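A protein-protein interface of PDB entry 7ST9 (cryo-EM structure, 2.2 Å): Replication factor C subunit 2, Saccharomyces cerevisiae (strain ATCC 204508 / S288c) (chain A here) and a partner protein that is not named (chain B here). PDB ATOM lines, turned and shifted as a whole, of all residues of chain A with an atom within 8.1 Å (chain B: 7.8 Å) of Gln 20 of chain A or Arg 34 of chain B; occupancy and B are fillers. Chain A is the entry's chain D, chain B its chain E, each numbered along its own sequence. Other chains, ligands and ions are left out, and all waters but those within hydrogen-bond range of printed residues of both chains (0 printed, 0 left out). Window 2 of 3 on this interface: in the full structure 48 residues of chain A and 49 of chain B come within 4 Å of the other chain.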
ATOM      1  N   GLU A  19       2.437 -17.727   6.088  1.00  0.00           N
ATOM      2  CA  GLU A  19       1.008 -17.445   6.050  1.00  0.00           C
ATOM      3  C   GLU A  19       0.351 -18.138   4.861  1.00  0.00           C
ATOM      4  O   GLU A  19      -0.761 -18.654   4.967  1.00  0.00           O
ATOM      5  CB  GLU A  19       0.761 -15.937   5.982  1.00  0.00           C
ATOM      6  N   GLN A  20       1.050 -18.145   3.724  1.00  0.00           N
ATOM      7  CA  GLN A  20       0.509 -18.784   2.530  1.00  0.00           C
ATOM      8  C   GLN A  20       0.346 -20.285   2.723  1.00  0.00           C
ATOM      9  O   GLN A  20      -0.609 -20.877   2.207  1.00  0.00           O
ATOM     10  CB  GLN A  20       1.412 -18.500   1.329  1.00  0.00           C
ATOM     11  N   SER A  21       1.264 -20.919   3.458  1.00  0.00           N
ATOM     12  CA  SER A  21       1.177 -22.361   3.662  1.00  0.00           C
ATOM     13  C   SER A  21      -0.101 -22.737   4.403  1.00  0.00           C
ATOM     14  O   SER A  21      -0.771 -23.713   4.045  1.00  0.00           O
ATOM     15  CB  SER A  21       2.404 -22.855   4.427  1.00  0.00           C
ATOM     16  OG  SER A  21       2.365 -24.260   4.602  1.00  0.00           O
ATOM     17  N   LEU A  22      -0.456 -21.976   5.440  1.00  0.00           N
ATOM     18  CA  LEU A  22      -1.678 -22.269   6.182  1.00  0.00           C
ATOM     19  C   LEU A  22      -2.922 -21.989   5.349  1.00  0.00           C
ATOM     20  O   LEU A  22      -3.938 -22.674   5.509  1.00  0.00           O
ATOM     21  CB  LEU A  22      -1.714 -21.456   7.476  1.00  0.00           C
ATOM     22  CG  LEU A  22      -0.640 -21.799   8.511  1.00  0.00           C
ATOM     23  CD1 LEU A  22      -0.650 -20.789   9.647  1.00  0.00           C
ATOM     24  CD2 LEU A  22      -0.834 -23.210   9.045  1.00  0.00           C
ATOM     25  N   ALA A  23      -2.863 -20.996   4.462  1.00  0.00           N
ATOM     26  CA  ALA A  23      -3.985 -20.639   3.606  1.00  0.00           C
ATOM     27  C   ALA A  23      -4.007 -21.437   2.308  1.00  0.00           C
ATOM     28  O   ALA A  23      -4.597 -20.982   1.321  1.00  0.00           O
ATOM     29  CB  ALA A  23      -3.954 -19.140   3.298  1.00  0.00           C
ATOM     30  N   GLN A  24      -3.376 -22.611   2.287  1.00  0.00           N
ATOM     31  CA  GLN A  24      -3.322 -23.459   1.104  1.00  0.00           C
ATOM     32  C   GLN A  24      -4.221 -24.684   1.235  1.00  0.00           C
ATOM     33  O   GLN A  24      -4.013 -25.678   0.532  1.00  0.00           O
ATOM     34  CB  GLN A  24      -1.880 -23.888   0.832  1.00  0.00           C
ATOM     35  CG  GLN A  24      -1.630 -24.383  -0.587  1.00  0.00           C
ATOM     36  CD  GLN A  24      -1.334 -25.872  -0.649  1.00  0.00           C
ATOM     37  OE1 GLN A  24      -0.719 -26.434   0.259  1.00  0.00           O
ATOM     38  NE2 GLN A  24      -1.768 -26.516  -1.726  1.00  0.00           N
ATOM     39  N   GLN A  25      -5.215 -24.634   2.121  1.00  0.00           N
ATOM     40  CA  GLN A  25      -6.111 -25.756   2.342  1.00  0.00           C
ATOM     41  C   GLN A  25      -7.563 -25.299   2.290  1.00  0.00           C
ATOM     42  O   GLN A  25      -7.881 -24.189   2.732  1.00  0.00           O
ATOM     43  CB  GLN A  25      -5.837 -26.419   3.698  1.00  0.00           C
ATOM     44  CG  GLN A  25      -4.667 -27.384   3.698  1.00  0.00           C
ATOM     45  CD  GLN A  25      -5.091 -28.801   3.364  1.00  0.00           C
ATOM     46  OE1 GLN A  25      -5.730 -29.045   2.341  1.00  0.00           O
ATOM     47  NE2 GLN A  25      -4.743 -29.744   4.234  1.00  0.00           N
ATOM     48  N   PRO A  26      -8.463 -26.127   1.761  1.00  0.00           N
ATOM     49  CA  PRO A  26      -9.893 -25.823   1.885  1.00  0.00           C
ATOM     50  C   PRO A  26     -10.314 -25.780   3.346  1.00  0.00           C
ATOM     51  O   PRO A  26      -9.746 -26.464   4.201  1.00  0.00           O
ATOM     52  CB  PRO A  26     -10.571 -26.976   1.135  1.00  0.00           C
ATOM     53  CG  PRO A  26      -9.534 -27.488   0.201  1.00  0.00           C
ATOM     54  CD  PRO A  26      -8.223 -27.298   0.899  1.00  0.00           C
ATOM     55  N   GLN A 236     -17.231 -20.724   2.840  1.00  0.00           N
ATOM     56  CA  GLN A 236     -15.989 -20.381   2.153  1.00  0.00           C
ATOM     57  C   GLN A 236     -16.269 -19.765   0.787  1.00  0.00           C
ATOM     58  O   GLN A 236     -15.607 -18.803   0.385  1.00  0.00           O
ATOM     59  CB  GLN A 236     -15.102 -21.617   2.009  1.00  0.00           C
ATOM     60  CG  GLN A 236     -13.724 -21.314   1.433  1.00  0.00           C
ATOM     61  CD  GLN A 236     -12.862 -22.550   1.289  1.00  0.00           C
ATOM     62  OE1 GLN A 236     -13.285 -23.659   1.611  1.00  0.00           O
ATOM     63  NE2 GLN A 236     -11.643 -22.365   0.795  1.00  0.00           N
ATOM     64  N   LYS A 240     -15.162 -16.045  -0.370  1.00  0.00           N
ATOM     65  CA  LYS A 240     -14.378 -15.784  -1.573  1.00  0.00           C
ATOM     66  C   LYS A 240     -15.068 -14.761  -2.463  1.00  0.00           C
ATOM     67  O   LYS A 240     -14.424 -13.844  -2.988  1.00  0.00           O
ATOM     68  CB  LYS A 240     -14.143 -17.084  -2.342  1.00  0.00           C
ATOM     69  CG  LYS A 240     -12.990 -17.919  -1.817  1.00  0.00           C
ATOM     70  CD  LYS A 240     -12.817 -19.190  -2.631  1.00  0.00           C
ATOM     71  CE  LYS A 240     -11.597 -19.975  -2.182  1.00  0.00           C
ATOM     72  NZ  LYS A 240     -10.328 -19.364  -2.663  1.00  0.00           N
ATOM     73  N   LEU B  29     -13.312 -17.194  -7.832  1.00  0.00           N
ATOM     74  CA  LEU B  29     -12.649 -18.421  -7.402  1.00  0.00           C
ATOM     75  C   LEU B  29     -11.153 -18.380  -7.690  1.00  0.00           C
ATOM     76  O   LEU B  29     -10.361 -18.943  -6.927  1.00  0.00           O
ATOM     77  CB  LEU B  29     -13.279 -19.633  -8.086  1.00  0.00           C
ATOM     78  CG  LEU B  29     -14.577 -20.177  -7.484  1.00  0.00           C
ATOM     79  CD1 LEU B  29     -15.124 -21.303  -8.347  1.00  0.00           C
ATOM     80  CD2 LEU B  29     -14.363 -20.655  -6.055  1.00  0.00           C
ATOM     81  N   SER B  30     -10.749 -17.724  -8.774  1.00  0.00           N
ATOM     82  CA  SER B  30      -9.355 -17.699  -9.197  1.00  0.00           C
ATOM     83  C   SER B  30      -8.543 -16.599  -8.526  1.00  0.00           C
ATOM     84  O   SER B  30      -7.339 -16.496  -8.783  1.00  0.00           O
ATOM     85  CB  SER B  30      -9.272 -17.535 -10.718  1.00  0.00           C
ATOM     86  OG  SER B  30      -9.523 -16.193 -11.099  1.00  0.00           O
ATOM     87  N   ASP B  31      -9.164 -15.774  -7.681  1.00  0.00           N
ATOM     88  CA  ASP B  31      -8.425 -14.705  -7.015  1.00  0.00           C
ATOM     89  C   ASP B  31      -7.347 -15.275  -6.100  1.00  0.00           C
ATOM     90  O   ASP B  31      -6.184 -14.860  -6.156  1.00  0.00           O
ATOM     91  CB  ASP B  31      -9.390 -13.819  -6.224  1.00  0.00           C
ATOM     92  CG  ASP B  31      -9.081 -12.340  -6.367  1.00  0.00           C
ATOM     93  OD1 ASP B  31      -8.563 -11.931  -7.427  1.00  0.00           O
ATOM     94  OD2 ASP B  31      -9.360 -11.583  -5.414  1.00  0.00           O
ATOM     95  N   GLN B  32      -7.716 -16.234  -5.253  1.00  0.00           N
ATOM     96  CA  GLN B  32      -6.796 -16.888  -4.322  1.00  0.00           C
ATOM     97  C   GLN B  32      -6.961 -18.393  -4.487  1.00  0.00           C
ATOM     98  O   GLN B  32      -7.597 -19.055  -3.656  1.00  0.00           O
ATOM     99  CB  GLN B  32      -7.062 -16.457  -2.878  1.00  0.00           C
ATOM    100  CG  GLN B  32      -6.918 -14.960  -2.609  1.00  0.00           C
ATOM    101  CD  GLN B  32      -5.752 -14.324  -3.343  1.00  0.00           C
ATOM    102  OE1 GLN B  32      -5.887 -13.252  -3.935  1.00  0.00           O
ATOM    103  NE2 GLN B  32      -4.593 -14.970  -3.289  1.00  0.00           N
ATOM    104  N   PRO B  33      -6.395 -18.971  -5.551  1.00  0.00           N
ATOM    105  CA  PRO B  33      -6.619 -20.397  -5.828  1.00  0.00           C
ATOM    106  C   PRO B  33      -5.880 -21.340  -4.892  1.00  0.00           C
ATOM    107  O   PRO B  33      -5.978 -22.560  -5.076  1.00  0.00           O
ATOM    108  CB  PRO B  33      -6.117 -20.551  -7.270  1.00  0.00           C
ATOM    109  CG  PRO B  33      -5.084 -19.492  -7.420  1.00  0.00           C
ATOM    110  CD  PRO B  33      -5.514 -18.342  -6.551  1.00  0.00           C
ATOM    111  N   ARG B  34      -5.145 -20.830  -3.903  1.00  0.00           N
ATOM    112  CA  ARG B  34      -4.395 -21.713  -3.017  1.00  0.00           C
ATOM    113  C   ARG B  34      -5.326 -22.636  -2.239  1.00  0.00           C
ATOM    114  O   ARG B  34      -5.050 -23.834  -2.099  1.00  0.00           O
ATOM    115  CB  ARG B  34      -3.536 -20.886  -2.062  1.00  0.00           C
ATOM    116  CG  ARG B  34      -2.210 -20.440  -2.656  1.00  0.00           C
ATOM    117  CD  ARG B  34      -1.143 -20.276  -1.586  1.00  0.00           C
ATOM    118  NE  ARG B  34       0.172 -20.017  -2.160  1.00  0.00           N
ATOM    119  CZ  ARG B  34       0.522 -18.886  -2.758  1.00  0.00           C
ATOM    120  NH1 ARG B  34      -0.325 -17.876  -2.880  1.00  0.00           N
ATOM    121  NH2 ARG B  34       1.753 -18.765  -3.247  1.00  0.00           N
ATOM    122  N   ASP B  35      -6.436 -22.100  -1.730  1.00  0.00           N
ATOM    123  CA  ASP B  35      -7.409 -22.875  -0.969  1.00  0.00           C
ATOM    124  C   ASP B  35      -8.644 -23.220  -1.797  1.00  0.00           C
ATOM    125  O   ASP B  35      -9.756 -23.278  -1.261  1.00  0.00           O
ATOM    126  CB  ASP B  35      -7.813 -22.121   0.299  1.00  0.00           C
ATOM    127  CG  ASP B  35      -8.189 -20.677   0.028  1.00  0.00           C
ATOM    128  OD1 ASP B  35      -8.630 -20.377  -1.100  1.00  0.00           O
ATOM    129  OD2 ASP B  35      -8.043 -19.842   0.945  1.00  0.00           O
ATOM    130  N   LEU B  36      -8.468 -23.456  -3.089  1.00  0.00           N
ATOM    131  CA  LEU B  36      -9.588 -23.796  -3.959  1.00  0.00           C
ATOM    132  C   LEU B  36     -10.163 -25.149  -3.556  1.00  0.00           C
ATOM    133  O   LEU B  36      -9.429 -26.146  -3.564  1.00  0.00           O
ATOM    134  CB  LEU B  36      -9.125 -23.827  -5.413  1.00  0.00           C
ATOM    135  CG  LEU B  36     -10.179 -24.147  -6.477  1.00  0.00           C
ATOM    136  CD1 LEU B  36     -11.084 -22.952  -6.722  1.00  0.00           C
ATOM    137  CD2 LEU B  36      -9.509 -24.590  -7.769  1.00  0.00           C
ATOM    138  N   PRO B  37     -11.442 -25.243  -3.204  1.00  0.00           N
ATOM    139  CA  PRO B  37     -12.032 -26.550  -2.899  1.00  0.00           C
ATOM    140  C   PRO B  37     -12.295 -27.352  -4.168  1.00  0.00           C
ATOM    141  O   PRO B  37     -12.216 -26.848  -5.289  1.00  0.00           O
ATOM    142  CB  PRO B  37     -13.346 -26.204  -2.185  1.00  0.00           C
ATOM    143  CG  PRO B  37     -13.274 -24.742  -1.882  1.00  0.00           C
ATOM    144  CD  PRO B  37     -12.384 -24.150  -2.917  1.00  0.00           C
ATOM    145  N   ILE B  60      -5.748 -19.829 -13.577  1.00  0.00           N
ATOM    146  CA  ILE B  60      -4.923 -20.229 -12.441  1.00  0.00           C
ATOM    147  C   ILE B  60      -3.473 -20.432 -12.870  1.00  0.00           C
ATOM    148  O   ILE B  60      -2.544 -19.980 -12.191  1.00  0.00           O
ATOM    149  CB  ILE B  60      -5.499 -21.495 -11.781  1.00  0.00           C
ATOM    150  CG1 ILE B  60      -6.777 -21.153 -11.012  1.00  0.00           C
ATOM    151  CG2 ILE B  60      -4.469 -22.126 -10.852  1.00  0.00           C
ATOM    152  CD1 ILE B  60      -7.613 -22.358 -10.647  1.00  0.00           C
ATOM    153  N   LYS B 128      14.271 -18.668  -5.666  1.00  0.00           N
ATOM    154  CA  LYS B 128      14.387 -18.871  -4.232  1.00  0.00           C
ATOM    155  C   LYS B 128      15.046 -20.216  -3.932  1.00  0.00           C
ATOM    156  O   LYS B 128      15.192 -21.081  -4.799  1.00  0.00           O
ATOM    157  CB  LYS B 128      13.013 -18.795  -3.569  1.00  0.00           C
ATOM    158  CG  LYS B 128      12.310 -17.458  -3.746  1.00  0.00           C
ATOM    159  CD  LYS B 128      10.896 -17.498  -3.191  1.00  0.00           C
ATOM    160  CE  LYS B 128      10.136 -16.220  -3.508  1.00  0.00           C
ATOM    161  NZ  LYS B 128       8.733 -16.265  -3.012  1.00  0.00           N
ATOM    162  N   HIS B 133       6.056 -26.671  -3.990  1.00  0.00           N
ATOM    163  CA  HIS B 133       5.025 -27.678  -4.195  1.00  0.00           C
ATOM    164  C   HIS B 133       3.770 -27.030  -4.759  1.00  0.00           C
ATOM    165  O   HIS B 133       3.401 -25.919  -4.366  1.00  0.00           O
ATOM    166  CB  HIS B 133       4.698 -28.400  -2.883  1.00  0.00           C
ATOM    167  CG  HIS B 133       3.306 -28.946  -2.825  1.00  0.00           C
ATOM    168  ND1 HIS B 133       2.300 -28.348  -2.097  1.00  0.00           N
ATOM    169  CD2 HIS B 133       2.751 -30.039  -3.403  1.00  0.00           C
ATOM    170  CE1 HIS B 133       1.187 -29.047  -2.230  1.00  0.00           C
ATOM    171  NE2 HIS B 133       1.434 -30.078  -3.017  1.00  0.00           N
ATOM    172  N   TYR B 135      -0.352 -28.210  -6.073  1.00  0.00           N
ATOM    173  CA  TYR B 135      -1.345 -29.269  -6.186  1.00  0.00           C
ATOM    174  C   TYR B 135      -1.674 -29.539  -7.650  1.00  0.00           C
ATOM    175  O   TYR B 135      -1.642 -28.640  -8.496  1.00  0.00           O
ATOM    176  CB  TYR B 135      -2.615 -28.913  -5.405  1.00  0.00           C
ATOM    177  CG  TYR B 135      -3.381 -27.701  -5.902  1.00  0.00           C
ATOM    178  CD1 TYR B 135      -4.097 -27.739  -7.094  1.00  0.00           C
ATOM    179  CD2 TYR B 135      -3.413 -26.528  -5.159  1.00  0.00           C
ATOM    180  CE1 TYR B 135      -4.801 -26.637  -7.539  1.00  0.00           C
ATOM    181  CE2 TYR B 135      -4.117 -25.423  -5.596  1.00  0.00           C
ATOM    182  CZ  TYR B 135      -4.811 -25.484  -6.786  1.00  0.00           C
ATOM    183  OH  TYR B 135      -5.512 -24.384  -7.222  1.00  0.00           O
ATOM    184  N   SER B 162      -5.961 -33.800   0.010  1.00  0.00           N
ATOM    185  CA  SER B 162      -6.396 -32.503  -0.496  1.00  0.00           C
ATOM    186  C   SER B 162      -5.212 -31.599  -0.819  1.00  0.00           C
ATOM    187  O   SER B 162      -5.313 -30.735  -1.697  1.00  0.00           O
ATOM    188  CB  SER B 162      -7.314 -31.829   0.524  1.00  0.00           C
ATOM    189  OG  SER B 162      -7.743 -30.558   0.068  1.00  0.00           O
ATOM    190  N   LYS B 163      -4.087 -31.778  -0.123  1.00  0.00           N
ATOM    191  CA  LYS B 163      -2.921 -30.937  -0.373  1.00  0.00           C
ATOM    192  C   LYS B 163      -2.394 -31.123  -1.790  1.00  0.00           C
ATOM    193  O   LYS B 163      -2.008 -30.150  -2.448  1.00  0.00           O
ATOM    194  CB  LYS B 163      -1.821 -31.251   0.642  1.00  0.00           C
ATOM    195  CG  LYS B 163      -2.165 -30.891   2.080  1.00  0.00           C
ATOM    196  CD  LYS B 163      -1.692 -29.488   2.451  1.00  0.00           C
ATOM    197  CE  LYS B 163      -0.908 -29.484   3.757  1.00  0.00           C
ATOM    198  NZ  LYS B 163      -1.635 -30.146   4.875  1.00  0.00           N
ATOM    199  N   ARG B 166      -6.728 -31.476  -6.474  1.00  0.00           N
ATOM    200  CA  ARG B 166      -8.016 -30.791  -6.454  1.00  0.00           C
ATOM    201  C   ARG B 166      -8.833 -31.293  -7.634  1.00  0.00           C
ATOM    202  O   ARG B 166      -8.413 -31.144  -8.786  1.00  0.00           O
ATOM    203  CB  ARG B 166      -7.842 -29.270  -6.521  1.00  0.00           C
ATOM    204  CG  ARG B 166      -6.962 -28.686  -5.423  1.00  0.00           C
ATOM    205  CD  ARG B 166      -7.591 -28.840  -4.045  1.00  0.00           C
ATOM    206  NE  ARG B 166      -6.634 -28.589  -2.975  1.00  0.00           N
ATOM    207  CZ  ARG B 166      -6.209 -27.387  -2.611  1.00  0.00           C
ATOM    208  NH1 ARG B 166      -6.645 -26.288  -3.204  1.00  0.00           N
ATOM    209  NH2 ARG B 166      -5.323 -27.283  -1.624  1.00  0.00           N
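The guanidinium group (NH1) of Arg 166 of chain B is in hydrogen-bond range of the backbone carbonyl oxygen (O) of Arg 34 of chain B.
NE of Arg 166 of chain B is in hydrogen-bond range of O of Ser 162 of chain B.
O of Leu 36 of chain B lies within hydrogen-bond range of NH1 of Arg 166 of chain B, at 2.8 Å.
O of Pro 33 of chain B sits at hydrogen-bond distance from OH of Tyr 135 of chain B (2.9 Å).
O of Lys 163 of chain B sits close to NE2 of His 133 of chain B (3.5 Å).
Among the printed residues, pairs that only touch across the chains: Gln 20 of chain A with Arg 34 of chain B (3.9 Å), Ala 23 of chain A with Arg 34 of chain B (3.5 Å), Ala 23 of chain A with Asp 35 of chain B (3.6 Å), Gln 24 of chain A with His 133 of chain B (3.9 Å), Gln 24 of chain A with Tyr 135 of chain B (3.8 Å), Gln 24 of chain A with Lys 163 of chain B (3.7 Å), Gln 25 of chain A with Asp 35 of chain B (3.2 Å), Pro 26 of chain A with Leu 36 of chain B (3.998 Å), Pro 26 of chain A with Ser 162 of chain B (3.4 Å), Pro 26 of chain A with Arg 166 of chain B (3.8 Å) and Gln 236 of chain A with Pro 37 of chain B (3.7 Å).
Of chain B, only Arg 34 (3.9 Å) comes within 4 Å of Gln 20 of chain A.
No residue of chain B comes within 4 Å of Glu 19 of chain A.
Printed residues of chain B within 4 Å of Gln 24 of chain A: Arg 34 (3.4 Å), His 133 (3.9 Å), Tyr 135 (3.8 Å), Lys 163 (3.7 Å) and Arg 166 (3.0 Å).
Printed residues of chain A within 4 Å of Pro 37 of chain B: Gln 236.
Printed residues of chain A within 4 Å of Tyr 135 of chain B: Gln 24 (3.8 Å).
Printed residues of chain A within 4 Å of Asp 35 of chain B: Ala 23 (3.6 Å), Gln 25 (3.2 Å), Gln 236 (2.9 Å) and Lys 240 (2.5 Å).
Printed residues of chain A within 4 Å of Gln 32 of chain B: Lys 240.
The nearest residue of chain B that does not touch Gln 20 of chain A is Asp 35 of chain B (7.1 Å).
The nearest residue of chain A that does not touch Arg 34 of chain B is Gln 25 of chain A (4.3 Å).
The backbone carbonyl oxygen (O) of Gln 24 of chain A sits close to the backbone carbonyl oxygen (O) of Arg 34 of chain B, 3.4 Å away.
NZ of Lys 163 of chain B lies close to NE2 of Gln 25 of chain A (3.2 Å).
The side-chain amide nitrogen (NE2) of Gln 236 of chain A lies within hydrogen-bond range of the backbone carbonyl oxygen (O) of Asp 35 of chain B.
OD1 of Asp 35 of chain B is in salt-bridge range of NZ of Lys 240 of chain A, 2.5 Å away.
OG of Ser 162 of chain B is in hydrogen-bond range of OE1 of Gln 25 of chain A, 3.4 Å away.
The side-chain amino group (NZ) of Lys 240 of chain A is in hydrogen-bond range of the backbone carbonyl oxygen (O) of Gln 32 of chain B.
O of Gln 24 of chain A lies within hydrogen-bond range of NH2 of Arg 166 of chain B, 3.0 Å away.
Hydrophobic or aromatic side chains of chain A within 4 Å of the printed part of chain B: Pro 26.
Of the 16 printed residues of chain B, 10 touch a printed residue of chain A.
Printed residues of chain B that touch a printed residue of chain A: Gln 32, Arg 34, Asp 35, Leu 36, Pro 37, His 133, Tyr 135, Ser 162, Lys 163 and Arg 166.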
